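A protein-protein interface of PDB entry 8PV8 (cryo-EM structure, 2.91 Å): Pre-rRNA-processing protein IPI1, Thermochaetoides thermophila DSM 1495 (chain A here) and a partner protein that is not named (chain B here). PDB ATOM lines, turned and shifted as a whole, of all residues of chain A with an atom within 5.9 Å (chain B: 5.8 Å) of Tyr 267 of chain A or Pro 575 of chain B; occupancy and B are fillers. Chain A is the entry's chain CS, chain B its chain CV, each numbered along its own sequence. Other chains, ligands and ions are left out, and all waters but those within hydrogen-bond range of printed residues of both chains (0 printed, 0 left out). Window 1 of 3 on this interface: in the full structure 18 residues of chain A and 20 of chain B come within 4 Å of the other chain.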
ATOM      1  N   ASN A 254     -32.770 -23.660 -11.053  1.00  0.00           N
ATOM      2  CA  ASN A 254     -31.762 -24.269 -10.194  1.00  0.00           C
ATOM      3  C   ASN A 254     -32.245 -25.553  -9.529  1.00  0.00           C
ATOM      4  O   ASN A 254     -31.416 -26.390  -9.158  1.00  0.00           O
ATOM      5  CB  ASN A 254     -31.322 -23.270  -9.119  1.00  0.00           C
ATOM      6  CG  ASN A 254     -30.078 -23.716  -8.381  1.00  0.00           C
ATOM      7  OD1 ASN A 254     -29.152 -24.264  -8.977  1.00  0.00           O
ATOM      8  ND2 ASN A 254     -30.053 -23.490  -7.073  1.00  0.00           N
ATOM      9  N   PRO A 259     -27.465 -29.060 -13.375  1.00  0.00           N
ATOM     10  CA  PRO A 259     -26.461 -28.016 -13.132  1.00  0.00           C
ATOM     11  C   PRO A 259     -25.606 -27.763 -14.366  1.00  0.00           C
ATOM     12  O   PRO A 259     -25.047 -28.689 -14.957  1.00  0.00           O
ATOM     13  CB  PRO A 259     -25.629 -28.589 -11.978  1.00  0.00           C
ATOM     14  CG  PRO A 259     -26.522 -29.598 -11.330  1.00  0.00           C
ATOM     15  CD  PRO A 259     -27.297 -30.199 -12.455  1.00  0.00           C
ATOM     16  N   THR A 261     -22.982 -25.622 -14.234  1.00  0.00           N
ATOM     17  CA  THR A 261     -21.652 -25.258 -13.762  1.00  0.00           C
ATOM     18  C   THR A 261     -20.670 -26.395 -14.028  1.00  0.00           C
ATOM     19  O   THR A 261     -20.951 -27.547 -13.685  1.00  0.00           O
ATOM     20  CB  THR A 261     -21.678 -24.946 -12.268  1.00  0.00           C
ATOM     21  OG1 THR A 261     -22.666 -23.943 -12.004  1.00  0.00           O
ATOM     22  CG2 THR A 261     -20.321 -24.445 -11.797  1.00  0.00           C
ATOM     23  N   PRO A 264     -19.681 -29.520 -10.985  1.00  0.00           N
ATOM     24  CA  PRO A 264     -20.564 -29.200  -9.862  1.00  0.00           C
ATOM     25  C   PRO A 264     -20.266 -30.094  -8.670  1.00  0.00           C
ATOM     26  O   PRO A 264     -19.633 -31.146  -8.790  1.00  0.00           O
ATOM     27  CB  PRO A 264     -21.961 -29.463 -10.425  1.00  0.00           C
ATOM     28  CG  PRO A 264     -21.746 -30.555 -11.403  1.00  0.00           C
ATOM     29  CD  PRO A 264     -20.362 -30.367 -11.982  1.00  0.00           C
ATOM     30  N   PHE A 265     -20.720 -29.635  -7.501  1.00  0.00           N
ATOM     31  CA  PHE A 265     -20.535 -30.292  -6.207  1.00  0.00           C
ATOM     32  C   PHE A 265     -19.068 -30.493  -5.850  1.00  0.00           C
ATOM     33  O   PHE A 265     -18.733 -31.416  -5.103  1.00  0.00           O
ATOM     34  CB  PHE A 265     -21.274 -31.633  -6.139  1.00  0.00           C
ATOM     35  CG  PHE A 265     -22.696 -31.560  -6.603  1.00  0.00           C
ATOM     36  CD1 PHE A 265     -23.628 -30.818  -5.902  1.00  0.00           C
ATOM     37  CD2 PHE A 265     -23.101 -32.236  -7.742  1.00  0.00           C
ATOM     38  CE1 PHE A 265     -24.935 -30.747  -6.328  1.00  0.00           C
ATOM     39  CE2 PHE A 265     -24.410 -32.170  -8.171  1.00  0.00           C
ATOM     40  CZ  PHE A 265     -25.328 -31.424  -7.464  1.00  0.00           C
ATOM     41  N   ALA A 266     -18.179 -29.643  -6.370  1.00  0.00           N
ATOM     42  CA  ALA A 266     -16.774 -29.722  -5.989  1.00  0.00           C
ATOM     43  C   ALA A 266     -16.552 -29.186  -4.583  1.00  0.00           C
ATOM     44  O   ALA A 266     -15.616 -29.612  -3.898  1.00  0.00           O
ATOM     45  CB  ALA A 266     -15.910 -28.961  -6.993  1.00  0.00           C
ATOM     46  N   TYR A 267     -17.397 -28.254  -4.140  1.00  0.00           N
ATOM     47  CA  TYR A 267     -17.273 -27.714  -2.792  1.00  0.00           C
ATOM     48  C   TYR A 267     -17.713 -28.714  -1.732  1.00  0.00           C
ATOM     49  O   TYR A 267     -17.365 -28.549  -0.558  1.00  0.00           O
ATOM     50  CB  TYR A 267     -18.076 -26.412  -2.661  1.00  0.00           C
ATOM     51  CG  TYR A 267     -19.565 -26.529  -2.928  1.00  0.00           C
ATOM     52  CD1 TYR A 267     -20.065 -26.551  -4.226  1.00  0.00           C
ATOM     53  CD2 TYR A 267     -20.471 -26.597  -1.879  1.00  0.00           C
ATOM     54  CE1 TYR A 267     -21.421 -26.655  -4.467  1.00  0.00           C
ATOM     55  CE2 TYR A 267     -21.829 -26.697  -2.111  1.00  0.00           C
ATOM     56  CZ  TYR A 267     -22.297 -26.727  -3.406  1.00  0.00           C
ATOM     57  OH  TYR A 267     -23.648 -26.827  -3.639  1.00  0.00           O
ATOM     58  N   LEU A 268     -18.473 -29.742  -2.116  1.00  0.00           N
ATOM     59  CA  LEU A 268     -18.840 -30.788  -1.169  1.00  0.00           C
ATOM     60  C   LEU A 268     -17.665 -31.704  -0.852  1.00  0.00           C
ATOM     61  O   LEU A 268     -17.427 -32.015   0.320  1.00  0.00           O
ATOM     62  CB  LEU A 268     -20.010 -31.605  -1.713  1.00  0.00           C
ATOM     63  CG  LEU A 268     -21.273 -30.830  -2.073  1.00  0.00           C
ATOM     64  CD1 LEU A 268     -22.356 -31.769  -2.565  1.00  0.00           C
ATOM     65  CD2 LEU A 268     -21.745 -30.062  -0.868  1.00  0.00           C
ATOM     66  N   ASN A 269     -16.924 -32.131  -1.883  1.00  0.00           N
ATOM     67  CA  ASN A 269     -15.810 -33.081  -1.759  1.00  0.00           C
ATOM     68  C   ASN A 269     -16.242 -34.363  -1.047  1.00  0.00           C
ATOM     69  O   ASN A 269     -15.546 -34.878  -0.170  1.00  0.00           O
ATOM     70  CB  ASN A 269     -14.605 -32.446  -1.058  1.00  0.00           C
ATOM     71  CG  ASN A 269     -13.313 -33.189  -1.332  1.00  0.00           C
ATOM     72  OD1 ASN A 269     -13.116 -33.739  -2.416  1.00  0.00           O
ATOM     73  ND2 ASN A 269     -12.436 -33.233  -0.338  1.00  0.00           N
ATOM     74  N   ARG A 275      -9.254 -32.277   2.218  1.00  0.00           N
ATOM     75  CA  ARG A 275      -8.421 -31.189   1.726  1.00  0.00           C
ATOM     76  C   ARG A 275      -7.840 -30.409   2.896  1.00  0.00           C
ATOM     77  O   ARG A 275      -8.563 -30.053   3.832  1.00  0.00           O
ATOM     78  CB  ARG A 275      -9.227 -30.256   0.819  1.00  0.00           C
ATOM     79  CG  ARG A 275      -9.977 -30.970  -0.290  1.00  0.00           C
ATOM     80  CD  ARG A 275     -10.046 -30.129  -1.551  1.00  0.00           C
ATOM     81  NE  ARG A 275     -11.137 -29.163  -1.500  1.00  0.00           N
ATOM     82  CZ  ARG A 275     -12.302 -29.317  -2.113  1.00  0.00           C
ATOM     83  NH1 ARG A 275     -12.561 -30.386  -2.847  1.00  0.00           N
ATOM     84  NH2 ARG A 275     -13.231 -28.373  -1.988  1.00  0.00           N
ATOM     85  N   MET A 281     -10.365 -24.900  -1.789  1.00  0.00           N
ATOM     86  CA  MET A 281     -10.762 -23.969  -2.833  1.00  0.00           C
ATOM     87  C   MET A 281     -11.302 -22.689  -2.207  1.00  0.00           C
ATOM     88  O   MET A 281     -11.994 -22.728  -1.184  1.00  0.00           O
ATOM     89  CB  MET A 281     -11.790 -24.613  -3.769  1.00  0.00           C
ATOM     90  CG  MET A 281     -13.129 -24.968  -3.143  1.00  0.00           C
ATOM     91  SD  MET A 281     -14.264 -25.704  -4.333  1.00  0.00           S
ATOM     92  CE  MET A 281     -14.686 -24.277  -5.328  1.00  0.00           C
ATOM     93  N   PRO B 539     -18.771 -19.024   1.932  1.00  0.00           N
ATOM     94  CA  PRO B 539     -18.976 -20.251   1.142  1.00  0.00           C
ATOM     95  C   PRO B 539     -18.510 -21.514   1.845  1.00  0.00           C
ATOM     96  O   PRO B 539     -19.076 -22.592   1.611  1.00  0.00           O
ATOM     97  CB  PRO B 539     -18.168 -19.980  -0.135  1.00  0.00           C
ATOM     98  CG  PRO B 539     -17.169 -18.945   0.259  1.00  0.00           C
ATOM     99  CD  PRO B 539     -17.858 -18.082   1.264  1.00  0.00           C
ATOM    100  N   ARG B 542     -21.378 -22.631   4.130  1.00  0.00           N
ATOM    101  CA  ARG B 542     -22.444 -23.249   3.346  1.00  0.00           C
ATOM    102  C   ARG B 542     -22.044 -24.639   2.863  1.00  0.00           C
ATOM    103  O   ARG B 542     -22.861 -25.570   2.882  1.00  0.00           O
ATOM    104  CB  ARG B 542     -22.809 -22.353   2.161  1.00  0.00           C
ATOM    105  CG  ARG B 542     -23.965 -22.861   1.308  1.00  0.00           C
ATOM    106  CD  ARG B 542     -25.178 -23.226   2.154  1.00  0.00           C
ATOM    107  NE  ARG B 542     -26.223 -23.866   1.365  1.00  0.00           N
ATOM    108  CZ  ARG B 542     -27.337 -23.267   0.968  1.00  0.00           C
ATOM    109  NH1 ARG B 542     -27.593 -22.007   1.280  1.00  0.00           N
ATOM    110  NH2 ARG B 542     -28.216 -23.948   0.241  1.00  0.00           N
ATOM    111  N   GLY B 543     -20.789 -24.796   2.437  1.00  0.00           N
ATOM    112  CA  GLY B 543     -20.309 -26.111   2.042  1.00  0.00           C
ATOM    113  C   GLY B 543     -20.301 -27.102   3.189  1.00  0.00           C
ATOM    114  O   GLY B 543     -20.687 -28.260   3.020  1.00  0.00           O
ATOM    115  N   ASP B 546     -23.921 -28.134   3.861  1.00  0.00           N
ATOM    116  CA  ASP B 546     -24.408 -29.082   2.862  1.00  0.00           C
ATOM    117  C   ASP B 546     -23.792 -30.465   3.053  1.00  0.00           C
ATOM    118  O   ASP B 546     -24.492 -31.480   2.930  1.00  0.00           O
ATOM    119  CB  ASP B 546     -24.121 -28.551   1.460  1.00  0.00           C
ATOM    120  CG  ASP B 546     -24.876 -27.275   1.157  1.00  0.00           C
ATOM    121  OD1 ASP B 546     -25.599 -26.785   2.049  1.00  0.00           O
ATOM    122  OD2 ASP B 546     -24.750 -26.763   0.026  1.00  0.00           O
ATOM    123  N   ARG B 547     -22.488 -30.522   3.356  1.00  0.00           N
ATOM    124  CA  ARG B 547     -21.842 -31.794   3.672  1.00  0.00           C
ATOM    125  C   ARG B 547     -22.493 -32.459   4.871  1.00  0.00           C
ATOM    126  O   ARG B 547     -22.738 -33.670   4.859  1.00  0.00           O
ATOM    127  CB  ARG B 547     -20.358 -31.595   3.969  1.00  0.00           C
ATOM    128  CG  ARG B 547     -19.475 -31.206   2.816  1.00  0.00           C
ATOM    129  CD  ARG B 547     -18.044 -31.082   3.312  1.00  0.00           C
ATOM    130  NE  ARG B 547     -17.473 -32.389   3.618  1.00  0.00           N
ATOM    131  CZ  ARG B 547     -17.204 -32.824   4.841  1.00  0.00           C
ATOM    132  NH1 ARG B 547     -17.435 -32.075   5.907  1.00  0.00           N
ATOM    133  NH2 ARG B 547     -16.695 -34.042   5.000  1.00  0.00           N
ATOM    134  N   TYR B 573     -26.423 -19.098  -8.826  1.00  0.00           N
ATOM    135  CA  TYR B 573     -26.752 -20.012  -7.748  1.00  0.00           C
ATOM    136  C   TYR B 573     -25.835 -21.233  -7.757  1.00  0.00           C
ATOM    137  O   TYR B 573     -25.380 -21.704  -8.804  1.00  0.00           O
ATOM    138  CB  TYR B 573     -28.204 -20.466  -7.851  1.00  0.00           C
ATOM    139  CG  TYR B 573     -29.238 -19.362  -7.782  1.00  0.00           C
ATOM    140  CD1 TYR B 573     -29.666 -18.703  -8.925  1.00  0.00           C
ATOM    141  CD2 TYR B 573     -29.790 -18.989  -6.568  1.00  0.00           C
ATOM    142  CE1 TYR B 573     -30.618 -17.711  -8.855  1.00  0.00           C
ATOM    143  CE2 TYR B 573     -30.741 -17.998  -6.490  1.00  0.00           C
ATOM    144  CZ  TYR B 573     -31.156 -17.372  -7.641  1.00  0.00           C
ATOM    145  OH  TYR B 573     -32.101 -16.381  -7.584  1.00  0.00           O
ATOM    146  N   TYR B 574     -25.568 -21.744  -6.564  1.00  0.00           N
ATOM    147  CA  TYR B 574     -24.880 -23.012  -6.411  1.00  0.00           C
ATOM    148  C   TYR B 574     -25.784 -24.151  -6.868  1.00  0.00           C
ATOM    149  O   TYR B 574     -27.011 -24.023  -6.849  1.00  0.00           O
ATOM    150  CB  TYR B 574     -24.474 -23.210  -4.954  1.00  0.00           C
ATOM    151  CG  TYR B 574     -23.116 -22.648  -4.600  1.00  0.00           C
ATOM    152  CD1 TYR B 574     -22.647 -21.477  -5.184  1.00  0.00           C
ATOM    153  CD2 TYR B 574     -22.311 -23.277  -3.662  1.00  0.00           C
ATOM    154  CE1 TYR B 574     -21.404 -20.959  -4.855  1.00  0.00           C
ATOM    155  CE2 TYR B 574     -21.068 -22.766  -3.324  1.00  0.00           C
ATOM    156  CZ  TYR B 574     -20.619 -21.606  -3.923  1.00  0.00           C
ATOM    157  OH  TYR B 574     -19.385 -21.089  -3.595  1.00  0.00           O
ATOM    158  N   PRO B 575     -25.203 -25.264  -7.324  1.00  0.00           N
ATOM    159  CA  PRO B 575     -26.021 -26.443  -7.644  1.00  0.00           C
ATOM    160  C   PRO B 575     -26.733 -26.986  -6.413  1.00  0.00           C
ATOM    161  O   PRO B 575     -26.218 -26.934  -5.294  1.00  0.00           O
ATOM    162  CB  PRO B 575     -24.998 -27.445  -8.191  1.00  0.00           C
ATOM    163  CG  PRO B 575     -23.888 -26.593  -8.702  1.00  0.00           C
ATOM    164  CD  PRO B 575     -23.809 -25.427  -7.766  1.00  0.00           C
ATOM    165  N   SER B 576     -27.936 -27.508  -6.633  1.00  0.00           N
ATOM    166  CA  SER B 576     -28.804 -27.905  -5.534  1.00  0.00           C
ATOM    167  C   SER B 576     -28.487 -29.319  -5.062  1.00  0.00           C
ATOM    168  O   SER B 576     -28.006 -30.156  -5.829  1.00  0.00           O
ATOM    169  CB  SER B 576     -30.270 -27.809  -5.955  1.00  0.00           C
ATOM    170  OG  SER B 576     -31.128 -28.233  -4.912  1.00  0.00           O
ATOM    171  N   ILE B 577     -28.776 -29.574  -3.783  1.00  0.00           N
ATOM    172  CA  ILE B 577     -28.493 -30.862  -3.149  1.00  0.00           C
ATOM    173  C   ILE B 577     -29.375 -31.969  -3.718  1.00  0.00           C
ATOM    174  O   ILE B 577     -28.962 -33.137  -3.768  1.00  0.00           O
ATOM    175  CB  ILE B 577     -28.636 -30.705  -1.614  1.00  0.00           C
ATOM    176  CG1 ILE B 577     -27.416 -29.972  -1.052  1.00  0.00           C
ATOM    177  CG2 ILE B 577     -28.848 -32.031  -0.882  1.00  0.00           C
ATOM    178  CD1 ILE B 577     -27.332 -29.979   0.457  1.00  0.00           C
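The guanidinium group of Arg 547 of chain B lies close to the backbone carbonyl oxygen of Leu 268 of chain A. The backbone carbonyl oxygen of Tyr 574 of chain B sits close to the side-chain amide oxygen of Asn 254 of chain A (3.0 Å). The backbone carbonyl oxygen of Pro 575 of chain B is in hydrogen-bond range of the side-chain hydroxyl of Tyr 267 of chain A.
The guanidinium group (NE) of Arg 542 of chain B is in salt-bridge range of the side-chain carboxylate (OD1) of Asp 546 of chain B (3.1 Å).
Hydrophobic or aromatic side chains of chain B within 4 Å of the printed part of chain A: Tyr 573, Tyr 574 and Pro 575. Printed residues of chain A that touch a printed residue of chain B: Asn 254, Pro 264, Phe 265, Tyr 267 and Leu 268. Among the printed residues, no Asp or Glu carboxylate lies within 4 Å of a Lys or Arg side-chain nitrogen of the other chain.
Printed residues of chain B within 4 Å of Asn 254 of chain A: Tyr 573 (3.6 Å), Tyr 574 (3.0 Å) and Ser 576 (3.7 Å). Printed residues of chain B within 4 Å of Phe 265 of chain A: Pro 575 (3.8 Å) and Ser 576 (3.2 Å). Of the printed residues of chain B, Tyr 267 of chain A touches Gly 543 (3.95 Å), Asp 546 (3.6 Å), Tyr 574 (3.5 Å) and Pro 575 (3.1 Å). Met 281 of chain A touches none of the printed residues of chain B. Printed residues of chain A within 4 Å of Gly 543 of chain B: Tyr 267. Of the printed residues of chain A, Tyr 573 of chain B touches Asn 254. Of the printed residues of chain A, Ser 576 of chain B touches Asn 254 and Phe 265. Ile 577 of chain B touches none of the printed residues of chain A. The nearest printed residue of chain A that does not touch Tyr 574 of chain B is Met 281 of chain A (5.9 Å).
Asn 254 of chain A touches Tyr 573 of chain B (ND2 to CB, 3.6 Å). O of Asn 254 of chain A touches CB of Ser 576 of chain B, at 3.7 Å. CB of Pro 264 of chain A touches CG of Pro 575 of chain B, 3.9 Å away. Phe 265 of chain A touches Pro 575 of chain B. O of Ser 576 of chain B touches CE1 of Phe 265 of chain A, 3.2 Å away. Tyr 267 of chain A touches Gly 543 of chain B. Asp 546 of chain B touches Tyr 267 of chain A (OD2 to CE2, 3.6 Å). CD2 of Tyr 574 of chain B touches CZ of Tyr 267 of chain A, 3.5 Å away. Leu 268 of chain A touches Asp 546 of chain B.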
